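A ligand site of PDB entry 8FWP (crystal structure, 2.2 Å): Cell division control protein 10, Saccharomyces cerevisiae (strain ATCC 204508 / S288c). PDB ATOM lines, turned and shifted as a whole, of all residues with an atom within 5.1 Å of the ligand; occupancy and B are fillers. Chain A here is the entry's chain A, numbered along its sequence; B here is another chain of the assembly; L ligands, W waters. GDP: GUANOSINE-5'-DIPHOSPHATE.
OG of Ser 23 lies close to N of Ser 37, at 3.3 Å. NE2 of His 158 of chain B is in hydrogen-bond range of OG of Ser 37 (3.4 Å). The side-chain amino group of Lys 22 sits at hydrogen-bond distance from the backbone carbonyl oxygen of Gln 17 (2.9 Å). O of Ile 186 of chain B sits at hydrogen-bond distance from NH2 of Arg 228 (2.9 Å). The side-chain amino group (NZ) of Lys 157 of chain A lies close to the backbone carbonyl oxygen (O) of Gly 19 (3.3 Å). The backbone NH (N) of His 158 of chain B sits at hydrogen-bond distance from the side-chain hydroxyl (OG1) of Thr 156 of chain B (3.0 Å). The side-chain carboxylate (OE1) of Glu 191 of chain B lies within salt-bridge range of the guanidinium group (NH2) of Arg 228 (2.9 Å). NZ of Lys 157 of chain A lies within hydrogen-bond range of O of Thr 156 of chain B (2.9 Å).
The backbone NH of Thr 24 is in hydrogen-bond range of an oxygen (O1A) of the ligand. O1A of the ligand sits at hydrogen-bond distance from OG1 of Thr 24 (2.6 Å). OD1 of Asp 159 is in hydrogen-bond range of N1 of the ligand, 2.7 Å away. The backbone NH of Ser 23 is in hydrogen-bond range of an oxygen (O3B) of the ligand (2.8 Å). An oxygen (O3B) of the ligand lies within hydrogen-bond range of the side-chain hydroxyl (OG) of Ser 23. OG of Ser 37 is in hydrogen-bond range of O2B of the ligand, 2.8 Å away. N of Gly 213 lies within hydrogen-bond range of O6 of the ligand (2.8 Å). The backbone NH (N) of Lys 22 lies within hydrogen-bond range of an oxygen (O1B) of the ligand. An oxygen (O1B) of the ligand is in salt-bridge range of the side-chain amino group (NZ) of Lys 22, 2.9 Å away. The backbone carbonyl oxygen of Ile 186 of chain B is in hydrogen-bond range of a nitrogen (N2) of the ligand (2.9 Å). The backbone NH (N) of Gly 19 lies within hydrogen-bond range of an oxygen (O2B) of the ligand (2.9 Å). A ring nitrogen (NE2) of His 158 of chain B lies within hydrogen-bond range of an oxygen (O2B) of the ligand, 3.0 Å away. An oxygen (O3A) of the ligand sits at hydrogen-bond distance from the backbone NH (N) of Gly 21, at 3.0 Å. O2' of the ligand sits at hydrogen-bond distance from OE2 of Glu 191 of chain B (3.0 Å). The side-chain amino group of Lys 157 of chain A lies close to an oxygen (O4') of the ligand (3.2 Å). A nitrogen (N3) of the ligand sits close to the guanidinium group (NH2) of Arg 228, at 3.4 Å. N of Leu 20 is in hydrogen-bond range of O1B of the ligand, 3.2 Å away.
Water W6 lies within hydrogen-bond range of the side-chain carboxylate (OD2) of Asp 74, an oxygen (O3B) of the ligand and the backbone NH (N) of Ala 38. Water W4 lies within hydrogen-bond range of a nitrogen (N7) of the ligand (2.9 Å), the backbone carbonyl oxygen of Gly 21 (3.0 Å) and the backbone NH of Gly 213 (3.4 Å). Water W1 lies within hydrogen-bond range of N3 of the ligand (2.9 Å), NZ of Lys 157 of chain A (3.1 Å) and OE1 of Glu 191 of chain B (3.2 Å). Water W3 lies within hydrogen-bond range of OG1 of Thr 39, O2B of the ligand and OG of Ser 37. Water W7 bridges OE2 of Glu 191 of chain B (2.7 Å) and O2' of the ligand (3.2 Å). Water W2 lies within hydrogen-bond range of OD2 of Asp 159 (2.7 Å), NE of Arg 228 (2.9 Å), O of Ile 186 of chain B (3.3 Å) and N2 of the ligand (3.5 Å).
Merely in contact with the ligand: Val 212 (3.2 Å) and Thr 156 of chain B (3.3 Å). Hydrophobic or aromatic side chains that line the ligand: Val 212, His 158 of chain B and Ile 186 of chain B. Of the 26 residues printed, 16 come within 4 Å of the ligand. The nearest printed residue that does not touch the ligand is Ser 18 (4.04 Å).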
ATOM      1  N   GLN A  17     -20.978  28.952 -14.188  1.00  0.00           N
ATOM      2  CA  GLN A  17     -20.889  27.517 -14.085  1.00  0.00           C
ATOM      3  C   GLN A  17     -21.612  27.033 -12.841  1.00  0.00           C
ATOM      4  O   GLN A  17     -21.919  27.795 -11.929  1.00  0.00           O
ATOM      5  CB  GLN A  17     -19.416  27.114 -14.106  1.00  0.00           C
ATOM      6  CG  GLN A  17     -18.709  27.741 -15.322  1.00  0.00           C
ATOM      7  CD  GLN A  17     -17.216  27.494 -15.367  1.00  0.00           C
ATOM      8  OE1 GLN A  17     -16.720  26.499 -14.843  1.00  0.00           O
ATOM      9  NE2 GLN A  17     -16.495  28.412 -16.008  1.00  0.00           N
ATOM     10  N   SER A  18     -21.977  25.755 -12.848  1.00  0.00           N
ATOM     11  CA  SER A  18     -22.740  25.195 -11.742  1.00  0.00           C
ATOM     12  C   SER A  18     -21.908  25.218 -10.454  1.00  0.00           C
ATOM     13  O   SER A  18     -20.689  25.030 -10.480  1.00  0.00           O
ATOM     14  CB  SER A  18     -23.177  23.774 -12.105  1.00  0.00           C
ATOM     15  OG  SER A  18     -23.089  22.909 -10.995  1.00  0.00           O
ATOM     16  N   GLY A  19     -22.560  25.490  -9.337  1.00  0.00           N
ATOM     17  CA  GLY A  19     -21.830  25.435  -8.079  1.00  0.00           C
ATOM     18  C   GLY A  19     -20.974  26.639  -7.760  1.00  0.00           C
ATOM     19  O   GLY A  19     -20.038  26.515  -6.976  1.00  0.00           O
ATOM     20  N   LEU A  20     -21.262  27.803  -8.336  1.00  0.00           N
ATOM     21  CA  LEU A  20     -20.600  29.041  -7.940  1.00  0.00           C
ATOM     22  C   LEU A  20     -21.399  29.795  -6.873  1.00  0.00           C
ATOM     23  O   LEU A  20     -21.046  30.931  -6.537  1.00  0.00           O
ATOM     24  CB  LEU A  20     -20.383  29.933  -9.167  1.00  0.00           C
ATOM     25  CG  LEU A  20     -19.069  29.707  -9.926  1.00  0.00           C
ATOM     26  CD1 LEU A  20     -19.033  30.550 -11.147  1.00  0.00           C
ATOM     27  CD2 LEU A  20     -17.853  30.010  -9.069  1.00  0.00           C
ATOM     28  N   GLY A  21     -22.451  29.171  -6.336  1.00  0.00           N
ATOM     29  CA  GLY A  21     -23.305  29.829  -5.356  1.00  0.00           C
ATOM     30  C   GLY A  21     -24.394  30.695  -5.955  1.00  0.00           C
ATOM     31  O   GLY A  21     -24.881  31.596  -5.272  1.00  0.00           O
ATOM     32  N   LYS A  22     -24.803  30.444  -7.210  1.00  0.00           N
ATOM     33  CA  LYS A  22     -25.753  31.342  -7.845  1.00  0.00           C
ATOM     34  C   LYS A  22     -27.105  31.297  -7.138  1.00  0.00           C
ATOM     35  O   LYS A  22     -27.664  32.343  -6.780  1.00  0.00           O
ATOM     36  CB  LYS A  22     -25.875  31.038  -9.348  1.00  0.00           C
ATOM     37  CG  LYS A  22     -24.495  31.122 -10.072  1.00  0.00           C
ATOM     38  CD  LYS A  22     -24.612  30.880 -11.565  1.00  0.00           C
ATOM     39  CE  LYS A  22     -25.467  29.663 -11.880  1.00  0.00           C
ATOM     40  NZ  LYS A  22     -24.727  28.459 -11.510  1.00  0.00           N
ATOM     41  N   SER A  23     -27.619  30.101  -6.858  1.00  0.00           N
ATOM     42  CA  SER A  23     -28.945  30.052  -6.251  1.00  0.00           C
ATOM     43  C   SER A  23     -28.899  30.541  -4.797  1.00  0.00           C
ATOM     44  O   SER A  23     -29.807  31.245  -4.347  1.00  0.00           O
ATOM     45  CB  SER A  23     -29.563  28.649  -6.363  1.00  0.00           C
ATOM     46  OG  SER A  23     -28.748  27.685  -5.746  1.00  0.00           O
ATOM     47  N   THR A  24     -27.824  30.220  -4.068  1.00  0.00           N
ATOM     48  CA  THR A  24     -27.678  30.697  -2.692  1.00  0.00           C
ATOM     49  C   THR A  24     -27.636  32.217  -2.633  1.00  0.00           C
ATOM     50  O   THR A  24     -28.240  32.826  -1.735  1.00  0.00           O
ATOM     51  CB  THR A  24     -26.410  30.125  -2.063  1.00  0.00           C
ATOM     52  OG1 THR A  24     -26.532  28.699  -1.936  1.00  0.00           O
ATOM     53  CG2 THR A  24     -26.164  30.715  -0.689  1.00  0.00           C
ATOM     54  N   LEU A  25     -26.929  32.845  -3.581  1.00  0.00           N
ATOM     55  CA  LEU A  25     -26.836  34.306  -3.586  1.00  0.00           C
ATOM     56  C   LEU A  25     -28.223  34.930  -3.773  1.00  0.00           C
ATOM     57  O   LEU A  25     -28.601  35.848  -3.040  1.00  0.00           O
ATOM     58  CB  LEU A  25     -25.872  34.784  -4.669  1.00  0.00           C
ATOM     59  CG  LEU A  25     -25.620  36.309  -4.639  1.00  0.00           C
ATOM     60  CD1 LEU A  25     -25.301  36.773  -3.258  1.00  0.00           C
ATOM     61  CD2 LEU A  25     -24.505  36.693  -5.557  1.00  0.00           C
ATOM     62  N   SER A  37     -30.805  25.248  -6.559  1.00  0.00           N
ATOM     63  CA  SER A  37     -29.710  25.114  -7.512  1.00  0.00           C
ATOM     64  C   SER A  37     -30.216  24.428  -8.775  1.00  0.00           C
ATOM     65  O   SER A  37     -30.933  23.422  -8.704  1.00  0.00           O
ATOM     66  CB  SER A  37     -28.553  24.301  -6.911  1.00  0.00           C
ATOM     67  OG  SER A  37     -27.559  24.005  -7.899  1.00  0.00           O
ATOM     68  N   ALA A  38     -29.849  24.984  -9.937  1.00  0.00           N
ATOM     69  CA  ALA A  38     -30.353  24.455 -11.199  1.00  0.00           C
ATOM     70  C   ALA A  38     -29.884  23.025 -11.455  1.00  0.00           C
ATOM     71  O   ALA A  38     -30.613  22.238 -12.065  1.00  0.00           O
ATOM     72  CB  ALA A  38     -29.945  25.362 -12.359  1.00  0.00           C
ATOM     73  N   THR A  39     -28.682  22.646 -10.986  1.00  0.00           N
ATOM     74  CA  THR A  39     -28.213  21.262 -11.128  1.00  0.00           C
ATOM     75  C   THR A  39     -28.139  20.473  -9.817  1.00  0.00           C
ATOM     76  O   THR A  39     -28.361  19.260  -9.850  1.00  0.00           O
ATOM     77  CB  THR A  39     -26.842  21.216 -11.819  1.00  0.00           C
ATOM     78  OG1 THR A  39     -25.950  22.140 -11.177  1.00  0.00           O
ATOM     79  CG2 THR A  39     -26.997  21.621 -13.276  1.00  0.00           C
ATOM     80  N   ASP A  74     -32.172  31.426 -14.429  1.00  0.00           N
ATOM     81  CA  ASP A  74     -30.928  30.693 -14.298  1.00  0.00           C
ATOM     82  C   ASP A  74     -30.563  30.073 -15.653  1.00  0.00           C
ATOM     83  O   ASP A  74     -31.396  29.969 -16.561  1.00  0.00           O
ATOM     84  CB  ASP A  74     -31.039  29.616 -13.199  1.00  0.00           C
ATOM     85  CG  ASP A  74     -29.670  29.341 -12.485  1.00  0.00           C
ATOM     86  OD1 ASP A  74     -28.589  29.544 -13.100  1.00  0.00           O
ATOM     87  OD2 ASP A  74     -29.675  28.891 -11.294  1.00  0.00           O
ATOM     88  N   LYS A 157     -18.288  32.724  -4.531  1.00  0.00           N
ATOM     89  CA  LYS A 157     -17.598  32.119  -3.381  1.00  0.00           C
ATOM     90  C   LYS A 157     -16.341  32.900  -3.056  1.00  0.00           C
ATOM     91  O   LYS A 157     -15.241  32.363  -2.943  1.00  0.00           O
ATOM     92  CB  LYS A 157     -17.277  30.655  -3.652  1.00  0.00           C
ATOM     93  CG  LYS A 157     -18.496  29.776  -3.759  1.00  0.00           C
ATOM     94  CD  LYS A 157     -18.095  28.307  -4.021  1.00  0.00           C
ATOM     95  CE  LYS A 157     -19.292  27.385  -3.925  1.00  0.00           C
ATOM     96  NZ  LYS A 157     -18.855  25.968  -3.900  1.00  0.00           N
ATOM     97  N   SER A 158     -16.503  34.213  -2.944  1.00  0.00           N
ATOM     98  CA  SER A 158     -15.337  35.065  -2.851  1.00  0.00           C
ATOM     99  C   SER A 158     -14.567  34.831  -1.551  1.00  0.00           C
ATOM    100  O   SER A 158     -13.408  35.269  -1.446  1.00  0.00           O
ATOM    101  CB  SER A 158     -15.767  36.539  -2.992  1.00  0.00           C
ATOM    102  OG  SER A 158     -16.325  36.989  -1.791  1.00  0.00           O
ATOM    103  N   ASP A 159     -15.159  34.136  -0.580  1.00  0.00           N
ATOM    104  CA  ASP A 159     -14.414  33.747   0.616  1.00  0.00           C
ATOM    105  C   ASP A 159     -13.258  32.784   0.284  1.00  0.00           C
ATOM    106  O   ASP A 159     -12.474  32.427   1.173  1.00  0.00           O
ATOM    107  CB  ASP A 159     -15.337  33.123   1.687  1.00  0.00           C
ATOM    108  CG  ASP A 159     -16.197  31.965   1.150  1.00  0.00           C
ATOM    109  OD1 ASP A 159     -16.911  32.143   0.126  1.00  0.00           O
ATOM    110  OD2 ASP A 159     -16.152  30.864   1.759  1.00  0.00           O
ATOM    111  N   VAL A 211     -18.781  38.495  -3.036  1.00  0.00           N
ATOM    112  CA  VAL A 211     -19.993  38.095  -2.320  1.00  0.00           C
ATOM    113  C   VAL A 211     -19.743  36.788  -1.615  1.00  0.00           C
ATOM    114  O   VAL A 211     -18.974  35.945  -2.079  1.00  0.00           O
ATOM    115  CB  VAL A 211     -21.212  37.986  -3.264  1.00  0.00           C
ATOM    116  CG1 VAL A 211     -21.531  39.307  -3.908  1.00  0.00           C
ATOM    117  CG2 VAL A 211     -20.980  36.910  -4.356  1.00  0.00           C
ATOM    118  N   VAL A 212     -20.423  36.610  -0.481  1.00  0.00           N
ATOM    119  CA  VAL A 212     -20.585  35.330   0.193  1.00  0.00           C
ATOM    120  C   VAL A 212     -22.074  35.164   0.452  1.00  0.00           C
ATOM    121  O   VAL A 212     -22.748  36.109   0.886  1.00  0.00           O
ATOM    122  CB  VAL A 212     -19.816  35.256   1.525  1.00  0.00           C
ATOM    123  CG1 VAL A 212     -20.032  33.922   2.195  1.00  0.00           C
ATOM    124  CG2 VAL A 212     -18.327  35.559   1.317  1.00  0.00           C
ATOM    125  N   GLY A 213     -22.607  33.971   0.167  1.00  0.00           N
ATOM    126  CA  GLY A 213     -24.026  33.712   0.305  1.00  0.00           C
ATOM    127  C   GLY A 213     -24.312  32.652   1.345  1.00  0.00           C
ATOM    128  O   GLY A 213     -23.512  31.734   1.543  1.00  0.00           O
ATOM    129  N   ARG A 228     -21.761  31.177   7.581  1.00  0.00           N
ATOM    130  CA  ARG A 228     -21.237  29.831   7.416  1.00  0.00           C
ATOM    131  C   ARG A 228     -20.241  29.549   8.531  1.00  0.00           C
ATOM    132  O   ARG A 228     -19.402  30.387   8.869  1.00  0.00           O
ATOM    133  CB  ARG A 228     -20.601  29.656   6.034  1.00  0.00           C
ATOM    134  CG  ARG A 228     -21.603  29.825   4.872  1.00  0.00           C
ATOM    135  CD  ARG A 228     -20.928  30.032   3.515  1.00  0.00           C
ATOM    136  NE  ARG A 228     -19.980  28.967   3.211  1.00  0.00           N
ATOM    137  CZ  ARG A 228     -20.294  27.744   2.791  1.00  0.00           C
ATOM    138  NH1 ARG A 228     -21.539  27.413   2.472  1.00  0.00           N
ATOM    139  NH2 ARG A 228     -19.331  26.816   2.717  1.00  0.00           N
ATOM    140  N   THR B 156     -16.857  22.709  -5.933  1.00  0.00           N
ATOM    141  CA  THR B 156     -18.212  23.172  -6.178  1.00  0.00           C
ATOM    142  C   THR B 156     -19.140  22.781  -5.035  1.00  0.00           C
ATOM    143  O   THR B 156     -20.109  23.497  -4.749  1.00  0.00           O
ATOM    144  CB  THR B 156     -18.735  22.561  -7.484  1.00  0.00           C
ATOM    145  OG1 THR B 156     -18.675  21.124  -7.386  1.00  0.00           O
ATOM    146  CG2 THR B 156     -17.887  23.023  -8.658  1.00  0.00           C
ATOM    147  N   GLY B 157     -18.875  21.648  -4.390  1.00  0.00           N
ATOM    148  CA  GLY B 157     -19.846  20.982  -3.554  1.00  0.00           C
ATOM    149  C   GLY B 157     -20.851  20.088  -4.282  1.00  0.00           C
ATOM    150  O   GLY B 157     -21.595  19.348  -3.621  1.00  0.00           O
ATOM    151  N   HIS B 158     -20.871  20.093  -5.618  1.00  0.00           N
ATOM    152  CA  HIS B 158     -21.896  19.337  -6.336  1.00  0.00           C
ATOM    153  C   HIS B 158     -21.410  17.952  -6.770  1.00  0.00           C
ATOM    154  O   HIS B 158     -21.592  16.990  -6.017  1.00  0.00           O
ATOM    155  CB  HIS B 158     -22.412  20.133  -7.539  1.00  0.00           C
ATOM    156  CG  HIS B 158     -23.278  21.290  -7.163  1.00  0.00           C
ATOM    157  ND1 HIS B 158     -24.072  21.282  -6.034  1.00  0.00           N
ATOM    158  CD2 HIS B 158     -23.475  22.483  -7.765  1.00  0.00           C
ATOM    159  CE1 HIS B 158     -24.730  22.427  -5.959  1.00  0.00           C
ATOM    160  NE2 HIS B 158     -24.390  23.174  -6.999  1.00  0.00           N
ATOM    161  N   ILE B 186     -12.907  26.512   1.733  1.00  0.00           N
ATOM    162  CA  ILE B 186     -14.206  27.168   1.552  1.00  0.00           C
ATOM    163  C   ILE B 186     -15.407  26.258   1.838  1.00  0.00           C
ATOM    164  O   ILE B 186     -16.550  26.749   1.878  1.00  0.00           O
ATOM    165  CB  ILE B 186     -14.317  27.747   0.125  1.00  0.00           C
ATOM    166  CG1 ILE B 186     -14.489  26.646  -0.929  1.00  0.00           C
ATOM    167  CG2 ILE B 186     -13.105  28.604  -0.209  1.00  0.00           C
ATOM    168  CD1 ILE B 186     -15.036  27.198  -2.237  1.00  0.00           C
ATOM    169  N   LEU B 187     -15.194  24.968   2.084  1.00  0.00           N
ATOM    170  CA  LEU B 187     -16.286  24.019   2.257  1.00  0.00           C
ATOM    171  C   LEU B 187     -16.600  23.790   3.728  1.00  0.00           C
ATOM    172  O   LEU B 187     -15.695  23.627   4.552  1.00  0.00           O
ATOM    173  CB  LEU B 187     -15.942  22.671   1.600  1.00  0.00           C
ATOM    174  CG  LEU B 187     -15.740  22.696   0.079  1.00  0.00           C
ATOM    175  CD1 LEU B 187     -15.222  21.404  -0.500  1.00  0.00           C
ATOM    176  CD2 LEU B 187     -17.032  23.083  -0.591  1.00  0.00           C
ATOM    177  N   GLU B 191     -20.483  19.804   3.763  1.00  0.00           N
ATOM    178  CA  GLU B 191     -20.293  19.829   2.308  1.00  0.00           C
ATOM    179  C   GLU B 191     -19.171  18.903   1.884  1.00  0.00           C
ATOM    180  O   GLU B 191     -19.265  18.235   0.852  1.00  0.00           O
ATOM    181  CB  GLU B 191     -19.991  21.250   1.830  1.00  0.00           C
ATOM    182  CG  GLU B 191     -21.192  22.189   1.761  1.00  0.00           C
ATOM    183  CD  GLU B 191     -20.805  23.683   1.831  1.00  0.00           C
ATOM    184  OE1 GLU B 191     -19.588  24.028   1.882  1.00  0.00           O
ATOM    185  OE2 GLU B 191     -21.730  24.515   1.866  1.00  0.00           O
HETATM  186  PB  GDP L   1     -25.273  27.044  -7.736  1.00  0.00           P
HETATM  187  O1B GDP L   1     -24.488  27.981  -8.653  1.00  0.00           O
HETATM  188  O2B GDP L   1     -25.316  25.650  -8.330  1.00  0.00           O
HETATM  189  O3B GDP L   1     -26.699  27.530  -7.580  1.00  0.00           O
HETATM  190  O3A GDP L   1     -24.518  27.050  -6.343  1.00  0.00           O
HETATM  191  PA  GDP L   1     -25.220  26.787  -4.909  1.00  0.00           P
HETATM  192  O1A GDP L   1     -25.912  28.009  -4.404  1.00  0.00           O
HETATM  193  O2A GDP L   1     -26.077  25.580  -4.970  1.00  0.00           O
HETATM  194  O5' GDP L   1     -23.859  26.525  -4.069  1.00  0.00           O
HETATM  195  C5' GDP L   1     -23.067  25.343  -4.231  1.00  0.00           C
HETATM  196  C4' GDP L   1     -22.412  24.988  -2.891  1.00  0.00           C
HETATM  197  O4' GDP L   1     -21.623  26.074  -2.370  1.00  0.00           O
HETATM  198  C3' GDP L   1     -23.466  24.683  -1.850  1.00  0.00           C
HETATM  199  O3' GDP L   1     -22.947  23.663  -1.000  1.00  0.00           O
HETATM  200  C2' GDP L   1     -23.555  25.965  -1.056  1.00  0.00           C
HETATM  201  O2' GDP L   1     -24.016  25.709   0.268  1.00  0.00           O
HETATM  202  C1' GDP L   1     -22.135  26.480  -1.098  1.00  0.00           C
HETATM  203  N9  GDP L   1     -22.075  27.946  -1.132  1.00  0.00           N
HETATM  204  C8  GDP L   1     -23.051  28.769  -1.545  1.00  0.00           C
HETATM  205  N7  GDP L   1     -22.632  30.054  -1.474  1.00  0.00           N
HETATM  206  C5  GDP L   1     -21.368  30.058  -1.017  1.00  0.00           C
HETATM  207  C6  GDP L   1     -20.345  31.073  -0.707  1.00  0.00           C
HETATM  208  O6  GDP L   1     -20.583  32.283  -0.858  1.00  0.00           O
HETATM  209  N1  GDP L   1     -19.153  30.654  -0.244  1.00  0.00           N
HETATM  210  C2  GDP L   1     -18.863  29.360  -0.053  1.00  0.00           C
HETATM  211  N2  GDP L   1     -17.633  29.032   0.393  1.00  0.00           N
HETATM  212  N3  GDP L   1     -19.752  28.374  -0.301  1.00  0.00           N
HETATM  213  C4  GDP L   1     -20.998  28.666  -0.786  1.00  0.00           C
HETATM  214  O   HOH W   1     -18.858  25.701  -0.792  1.00  0.00           O
HETATM  215  O   HOH W   2     -17.174  29.381   3.800  1.00  0.00           O
HETATM  216  O   HOH W   3     -26.350  24.690 -10.872  1.00  0.00           O
HETATM  217  O   HOH W   4     -23.421  32.473  -2.778  1.00  0.00           O
HETATM  218  O   HOH W   5     -27.265  24.558  -3.000  1.00  0.00           O
HETATM  219  O   HOH W   6     -28.105  27.364 -10.023  1.00  0.00           O
HETATM  220  O   HOH W   7     -23.984  24.783   3.368  1.00  0.00           O
